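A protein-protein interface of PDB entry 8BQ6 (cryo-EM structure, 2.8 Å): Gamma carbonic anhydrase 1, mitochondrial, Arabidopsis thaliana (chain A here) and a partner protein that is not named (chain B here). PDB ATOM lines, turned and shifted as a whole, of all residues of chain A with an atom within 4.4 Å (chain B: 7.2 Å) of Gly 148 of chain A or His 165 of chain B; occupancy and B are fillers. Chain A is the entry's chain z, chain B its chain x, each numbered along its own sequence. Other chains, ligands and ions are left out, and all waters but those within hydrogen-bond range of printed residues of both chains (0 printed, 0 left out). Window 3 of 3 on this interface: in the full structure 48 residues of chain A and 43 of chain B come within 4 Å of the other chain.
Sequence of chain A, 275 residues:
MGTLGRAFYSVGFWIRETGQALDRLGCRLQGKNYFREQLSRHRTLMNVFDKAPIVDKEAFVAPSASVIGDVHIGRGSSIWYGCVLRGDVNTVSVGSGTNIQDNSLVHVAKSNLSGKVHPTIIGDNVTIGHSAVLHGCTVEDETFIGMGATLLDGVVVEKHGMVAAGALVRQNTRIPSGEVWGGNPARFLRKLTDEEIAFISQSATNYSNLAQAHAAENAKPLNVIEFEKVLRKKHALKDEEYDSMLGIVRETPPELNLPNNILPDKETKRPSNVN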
ATOM      1  N   HIS A 130      21.364  -3.100 -11.951  1.00  0.00           N
ATOM      2  CA  HIS A 130      19.916  -2.862 -12.139  1.00  0.00           C
ATOM      3  C   HIS A 130      19.062  -3.690 -11.191  1.00  0.00           C
ATOM      4  O   HIS A 130      19.294  -4.902 -11.115  1.00  0.00           O
ATOM      5  CB  HIS A 130      19.516  -3.210 -13.573  1.00  0.00           C
ATOM      6  CG  HIS A 130      20.337  -2.582 -14.645  1.00  0.00           C
ATOM      7  ND1 HIS A 130      20.168  -1.271 -15.032  1.00  0.00           N
ATOM      8  CD2 HIS A 130      21.284  -3.097 -15.455  1.00  0.00           C
ATOM      9  CE1 HIS A 130      20.998  -0.996 -16.015  1.00  0.00           C
ATOM     10  NE2 HIS A 130      21.695  -2.099 -16.292  1.00  0.00           N
ATOM     11  N   SER A 131      18.112  -3.053 -10.517  1.00  0.00           N
ATOM     12  CA  SER A 131      17.137  -3.707  -9.649  1.00  0.00           C
ATOM     13  C   SER A 131      17.802  -4.429  -8.485  1.00  0.00           C
ATOM     14  O   SER A 131      17.414  -5.543  -8.125  1.00  0.00           O
ATOM     15  CB  SER A 131      16.255  -4.670 -10.445  1.00  0.00           C
ATOM     16  OG  SER A 131      15.967  -4.139 -11.724  1.00  0.00           O
ATOM     17  N   ALA A 132      18.806  -3.797  -7.890  1.00  0.00           N
ATOM     18  CA  ALA A 132      19.469  -4.346  -6.722  1.00  0.00           C
ATOM     19  C   ALA A 132      18.884  -3.733  -5.457  1.00  0.00           C
ATOM     20  O   ALA A 132      18.398  -2.600  -5.460  1.00  0.00           O
ATOM     21  CB  ALA A 132      20.972  -4.087  -6.790  1.00  0.00           C
ATOM     22  N   VAL A 133      18.926  -4.497  -4.371  1.00  0.00           N
ATOM     23  CA  VAL A 133      18.322  -4.095  -3.107  1.00  0.00           C
ATOM     24  C   VAL A 133      19.415  -3.977  -2.059  1.00  0.00           C
ATOM     25  O   VAL A 133      20.030  -4.980  -1.677  1.00  0.00           O
ATOM     26  CB  VAL A 133      17.238  -5.082  -2.655  1.00  0.00           C
ATOM     27  CG1 VAL A 133      16.724  -4.700  -1.278  1.00  0.00           C
ATOM     28  CG2 VAL A 133      16.101  -5.103  -3.658  1.00  0.00           C
ATOM     29  N   GLY A 146      26.323  -6.967  -8.061  1.00  0.00           N
ATOM     30  CA  GLY A 146      25.606  -7.529  -9.172  1.00  0.00           C
ATOM     31  C   GLY A 146      24.151  -7.113  -9.171  1.00  0.00           C
ATOM     32  O   GLY A 146      23.523  -6.907  -8.131  1.00  0.00           O
ATOM     33  N   MET A 147      23.640  -6.969 -10.381  1.00  0.00           N
ATOM     34  CA  MET A 147      22.253  -6.652 -10.652  1.00  0.00           C
ATOM     35  C   MET A 147      21.324  -7.747 -10.123  1.00  0.00           C
ATOM     36  O   MET A 147      21.668  -8.930 -10.102  1.00  0.00           O
ATOM     37  CB  MET A 147      22.167  -6.373 -12.161  1.00  0.00           C
ATOM     38  CG  MET A 147      22.206  -7.581 -13.050  1.00  0.00           C
ATOM     39  SD  MET A 147      20.696  -8.472 -13.089  1.00  0.00           S
ATOM     40  CE  MET A 147      20.006  -7.547 -14.373  1.00  0.00           C
ATOM     41  N   GLY A 148      20.175  -7.324  -9.593  1.00  0.00           N
ATOM     42  CA  GLY A 148      19.224  -8.227  -8.966  1.00  0.00           C
ATOM     43  C   GLY A 148      19.637  -8.797  -7.624  1.00  0.00           C
ATOM     44  O   GLY A 148      18.912  -9.638  -7.081  1.00  0.00           O
ATOM     45  N   ALA A 149      20.772  -8.375  -7.074  1.00  0.00           N
ATOM     46  CA  ALA A 149      21.270  -8.895  -5.812  1.00  0.00           C
ATOM     47  C   ALA A 149      20.663  -8.137  -4.636  1.00  0.00           C
ATOM     48  O   ALA A 149      20.248  -6.982  -4.754  1.00  0.00           O
ATOM     49  CB  ALA A 149      22.793  -8.799  -5.757  1.00  0.00           C
ATOM     50  N   THR A 150      20.623  -8.800  -3.483  1.00  0.00           N
ATOM     51  CA  THR A 150      20.092  -8.205  -2.265  1.00  0.00           C
ATOM     52  C   THR A 150      21.151  -8.247  -1.174  1.00  0.00           C
ATOM     53  O   THR A 150      21.743  -9.300  -0.919  1.00  0.00           O
ATOM     54  CB  THR A 150      18.821  -8.925  -1.793  1.00  0.00           C
ATOM     55  OG1 THR A 150      17.826  -8.876  -2.823  1.00  0.00           O
ATOM     56  CG2 THR A 150      18.265  -8.275  -0.534  1.00  0.00           C
ATOM     57  N   GLY A 166      21.991 -11.593  -8.848  1.00  0.00           N
ATOM     58  CA  GLY A 166      20.997 -12.458  -8.248  1.00  0.00           C
ATOM     59  C   GLY A 166      21.353 -13.029  -6.894  1.00  0.00           C
ATOM     60  O   GLY A 166      20.622 -13.887  -6.394  1.00  0.00           O
ATOM     61  N   CYS B 121       7.119  -3.002  -4.935  1.00  0.00           N
ATOM     62  CA  CYS B 121       6.364  -4.240  -5.025  1.00  0.00           C
ATOM     63  C   CYS B 121       5.385  -4.175  -6.191  1.00  0.00           C
ATOM     64  O   CYS B 121       4.898  -3.107  -6.561  1.00  0.00           O
ATOM     65  CB  CYS B 121       5.593  -4.498  -3.730  1.00  0.00           C
ATOM     66  SG  CYS B 121       6.583  -4.935  -2.288  1.00  0.00           S
ATOM     67  N   GLY B 146       7.450  -7.259   2.306  1.00  0.00           N
ATOM     68  CA  GLY B 146       8.765  -6.673   2.146  1.00  0.00           C
ATOM     69  C   GLY B 146       8.995  -6.080   0.775  1.00  0.00           C
ATOM     70  O   GLY B 146       8.414  -6.536  -0.212  1.00  0.00           O
ATOM     71  N   ALA B 147       9.857  -5.069   0.709  1.00  0.00           N
ATOM     72  CA  ALA B 147      10.044  -4.299  -0.510  1.00  0.00           C
ATOM     73  C   ALA B 147      10.487  -5.187  -1.664  1.00  0.00           C
ATOM     74  O   ALA B 147      11.136  -6.218  -1.471  1.00  0.00           O
ATOM     75  CB  ALA B 147      11.077  -3.199  -0.274  1.00  0.00           C
ATOM     76  N   TYR B 148      10.120  -4.771  -2.877  1.00  0.00           N
ATOM     77  CA  TYR B 148      10.484  -5.442  -4.122  1.00  0.00           C
ATOM     78  C   TYR B 148       9.901  -6.841  -4.235  1.00  0.00           C
ATOM     79  O   TYR B 148      10.509  -7.717  -4.855  1.00  0.00           O
ATOM     80  CB  TYR B 148      12.005  -5.503  -4.295  1.00  0.00           C
ATOM     81  CG  TYR B 148      12.495  -4.851  -5.557  1.00  0.00           C
ATOM     82  CD1 TYR B 148      12.238  -5.418  -6.793  1.00  0.00           C
ATOM     83  CD2 TYR B 148      13.209  -3.665  -5.514  1.00  0.00           C
ATOM     84  CE1 TYR B 148      12.682  -4.826  -7.950  1.00  0.00           C
ATOM     85  CE2 TYR B 148      13.655  -3.066  -6.666  1.00  0.00           C
ATOM     86  CZ  TYR B 148      13.389  -3.652  -7.880  1.00  0.00           C
ATOM     87  OH  TYR B 148      13.832  -3.062  -9.036  1.00  0.00           O
ATOM     88  N   SER B 149       8.725  -7.070  -3.666  1.00  0.00           N
ATOM     89  CA  SER B 149       8.094  -8.379  -3.698  1.00  0.00           C
ATOM     90  C   SER B 149       7.035  -8.415  -4.791  1.00  0.00           C
ATOM     91  O   SER B 149       6.379  -7.408  -5.065  1.00  0.00           O
ATOM     92  CB  SER B 149       7.462  -8.694  -2.344  1.00  0.00           C
ATOM     93  OG  SER B 149       8.435  -9.132  -1.414  1.00  0.00           O
ATOM     94  N   LEU B 150       6.869  -9.575  -5.418  1.00  0.00           N
ATOM     95  CA  LEU B 150       5.879  -9.746  -6.471  1.00  0.00           C
ATOM     96  C   LEU B 150       4.807 -10.713  -5.995  1.00  0.00           C
ATOM     97  O   LEU B 150       5.115 -11.833  -5.575  1.00  0.00           O
ATOM     98  CB  LEU B 150       6.525 -10.246  -7.761  1.00  0.00           C
ATOM     99  CG  LEU B 150       7.872  -9.591  -8.066  1.00  0.00           C
ATOM    100  CD1 LEU B 150       8.528 -10.266  -9.246  1.00  0.00           C
ATOM    101  CD2 LEU B 150       7.728  -8.094  -8.299  1.00  0.00           C
ATOM    102  N   ILE B 162       6.378 -11.004   4.995  1.00  0.00           N
ATOM    103  CA  ILE B 162       6.937 -11.452   3.726  1.00  0.00           C
ATOM    104  C   ILE B 162       8.304 -10.800   3.575  1.00  0.00           C
ATOM    105  O   ILE B 162       8.416  -9.569   3.617  1.00  0.00           O
ATOM    106  CB  ILE B 162       6.029 -11.078   2.544  1.00  0.00           C
ATOM    107  CG1 ILE B 162       4.621 -11.659   2.707  1.00  0.00           C
ATOM    108  CG2 ILE B 162       6.645 -11.553   1.239  1.00  0.00           C
ATOM    109  CD1 ILE B 162       4.568 -13.146   2.826  1.00  0.00           C
ATOM    110  N   GLY B 163       9.342 -11.609   3.391  1.00  0.00           N
ATOM    111  CA  GLY B 163      10.680 -11.065   3.283  1.00  0.00           C
ATOM    112  C   GLY B 163      10.888 -10.264   2.013  1.00  0.00           C
ATOM    113  O   GLY B 163      10.211 -10.448   1.002  1.00  0.00           O
ATOM    114  N   GLN B 164      11.863  -9.359   2.075  1.00  0.00           N
ATOM    115  CA  GLN B 164      12.205  -8.530   0.926  1.00  0.00           C
ATOM    116  C   GLN B 164      12.544  -9.398  -0.280  1.00  0.00           C
ATOM    117  O   GLN B 164      13.118 -10.481  -0.151  1.00  0.00           O
ATOM    118  CB  GLN B 164      13.399  -7.637   1.257  1.00  0.00           C
ATOM    119  CG  GLN B 164      13.062  -6.365   1.998  1.00  0.00           C
ATOM    120  CD  GLN B 164      14.278  -5.484   2.192  1.00  0.00           C
ATOM    121  OE1 GLN B 164      14.617  -4.678   1.329  1.00  0.00           O
ATOM    122  NE2 GLN B 164      14.949  -5.643   3.325  1.00  0.00           N
ATOM    123  N   HIS B 165      12.164  -8.913  -1.463  1.00  0.00           N
ATOM    124  CA  HIS B 165      12.518  -9.547  -2.734  1.00  0.00           C
ATOM    125  C   HIS B 165      11.941 -10.955  -2.850  1.00  0.00           C
ATOM    126  O   HIS B 165      12.604 -11.870  -3.341  1.00  0.00           O
ATOM    127  CB  HIS B 165      14.038  -9.572  -2.927  1.00  0.00           C
ATOM    128  CG  HIS B 165      14.480  -9.149  -4.292  1.00  0.00           C
ATOM    129  ND1 HIS B 165      13.948  -9.680  -5.447  1.00  0.00           N
ATOM    130  CD2 HIS B 165      15.392  -8.231  -4.685  1.00  0.00           C
ATOM    131  CE1 HIS B 165      14.520  -9.112  -6.492  1.00  0.00           C
ATOM    132  NE2 HIS B 165      15.400  -8.227  -6.059  1.00  0.00           N
ATOM    133  N   SER B 166      10.703 -11.136  -2.405  1.00  0.00           N
ATOM    134  CA  SER B 166      10.048 -12.434  -2.422  1.00  0.00           C
ATOM    135  C   SER B 166       9.024 -12.506  -3.548  1.00  0.00           C
ATOM    136  O   SER B 166       8.559 -11.488  -4.066  1.00  0.00           O
ATOM    137  CB  SER B 166       9.370 -12.711  -1.083  1.00  0.00           C
ATOM    138  OG  SER B 166      10.327 -12.888  -0.056  1.00  0.00           O
ATOM    139  N   ILE B 167       8.668 -13.730  -3.920  1.00  0.00           N
ATOM    140  CA  ILE B 167       7.770 -13.977  -5.041  1.00  0.00           C
ATOM    141  C   ILE B 167       6.713 -14.973  -4.596  1.00  0.00           C
ATOM    142  O   ILE B 167       7.044 -16.092  -4.189  1.00  0.00           O
ATOM    143  CB  ILE B 167       8.526 -14.507  -6.267  1.00  0.00           C
ATOM    144  CG1 ILE B 167       9.489 -13.443  -6.780  1.00  0.00           C
ATOM    145  CG2 ILE B 167       7.558 -14.890  -7.363  1.00  0.00           C
ATOM    146  CD1 ILE B 167      10.243 -13.869  -7.982  1.00  0.00           C
ATOM    147  N   GLU B 181      11.583 -15.668   4.662  1.00  0.00           N
ATOM    148  CA  GLU B 181      12.829 -14.931   4.587  1.00  0.00           C
ATOM    149  C   GLU B 181      12.898 -14.122   3.303  1.00  0.00           C
ATOM    150  O   GLU B 181      12.125 -14.320   2.364  1.00  0.00           O
ATOM    151  CB  GLU B 181      14.035 -15.853   4.635  1.00  0.00           C
ATOM    152  CG  GLU B 181      14.096 -16.779   5.794  1.00  0.00           C
ATOM    153  CD  GLU B 181      15.474 -17.357   5.909  1.00  0.00           C
ATOM    154  OE1 GLU B 181      16.171 -17.022   6.886  1.00  0.00           O
ATOM    155  OE2 GLU B 181      15.886 -18.096   4.990  1.00  0.00           O
ATOM    156  N   ALA B 182      13.862 -13.207   3.268  1.00  0.00           N
ATOM    157  CA  ALA B 182      14.112 -12.446   2.057  1.00  0.00           C
ATOM    158  C   ALA B 182      14.545 -13.378   0.934  1.00  0.00           C
ATOM    159  O   ALA B 182      15.251 -14.363   1.159  1.00  0.00           O
ATOM    160  CB  ALA B 182      15.183 -11.387   2.308  1.00  0.00           C
ATOM    161  N   GLY B 183      14.102 -13.066  -0.281  1.00  0.00           N
ATOM    162  CA  GLY B 183      14.466 -13.844  -1.445  1.00  0.00           C
ATOM    163  C   GLY B 183      13.731 -15.152  -1.612  1.00  0.00           C
ATOM    164  O   GLY B 183      14.187 -16.006  -2.379  1.00  0.00           O
ATOM    165  N   SER B 184      12.610 -15.338  -0.926  1.00  0.00           N
ATOM    166  CA  SER B 184      11.853 -16.575  -1.023  1.00  0.00           C
ATOM    167  C   SER B 184      11.035 -16.612  -2.306  1.00  0.00           C
ATOM    168  O   SER B 184      10.649 -15.577  -2.853  1.00  0.00           O
ATOM    169  CB  SER B 184      10.929 -16.725   0.179  1.00  0.00           C
ATOM    170  OG  SER B 184      11.675 -16.730   1.380  1.00  0.00           O
ATOM    171  N   VAL B 185      10.768 -17.823  -2.781  1.00  0.00           N
ATOM    172  CA  VAL B 185      10.018 -18.047  -4.012  1.00  0.00           C
ATOM    173  C   VAL B 185       8.998 -19.144  -3.733  1.00  0.00           C
ATOM    174  O   VAL B 185       9.368 -20.302  -3.502  1.00  0.00           O
ATOM    175  CB  VAL B 185      10.944 -18.419  -5.179  1.00  0.00           C
ATOM    176  CG1 VAL B 185      10.145 -18.791  -6.404  1.00  0.00           C
ATOM    177  CG2 VAL B 185      11.872 -17.260  -5.504  1.00  0.00           C
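The backbone carbonyl oxygen (O) of Ala 147 of chain B lies within hydrogen-bond range of the backbone NH (N) of His 165 of chain B (2.9 Å).
The backbone NH (N) of Tyr 148 of chain B sits at hydrogen-bond distance from the side-chain sulfur (SG) of Cys 121 of chain B, 3.6 Å away.
O of Gln 164 of chain B lies within hydrogen-bond range of N of Gly 183 of chain B.
N of Val 133 of chain A sits at hydrogen-bond distance from O of Ala 149 of chain A (2.8 Å).
The backbone NH (N) of Gly 148 of chain A lies within hydrogen-bond range of the backbone carbonyl oxygen (O) of His 130 of chain A (3.0 Å).
Among the printed residues, merely in contact across the chains: Ser 131 of chain A with Tyr 148 of chain B, Ser 131 of chain A with His 165 of chain B, Val 133 of chain A with Tyr 148 of chain B, Val 133 of chain A with Gln 164 of chain B, Val 133 of chain A with His 165 of chain B, Gly 148 of chain A with His 165 of chain B and Thr 150 of chain A with His 165 of chain B.
Of the printed residues of chain B, Ser 131 of chain A touches Tyr 148 (3.2 Å) and His 165 (3.9 Å).
Printed residues of chain B within 4 Å of Val 133 of chain A: Tyr 148, Gln 164 and His 165.
Of chain B, only His 165 comes within 4 Å of Gly 148 of chain A.
Of the printed residues of chain B, Thr 150 of chain A touches His 165 (3.1 Å).
Of the printed residues of chain A, Tyr 148 of chain B touches Ser 131 and Val 133.
Of the printed residues of chain A, Gln 164 of chain B touches Val 133 (3.4 Å).
His 165 of chain B touches four residues of chain A.
Of the 10 printed residues of chain A, 4 touch a printed residue of chain B.
Printed residues of chain A that touch a printed residue of chain B: Ser 131, Val 133, Gly 148 and Thr 150.
Of the 17 printed residues of chain B, 3 touch a printed residue of chain A.
Among the printed residues, no Asp or Glu carboxylate lies within 4 Å of a Lys or Arg side-chain nitrogen of the other chain.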
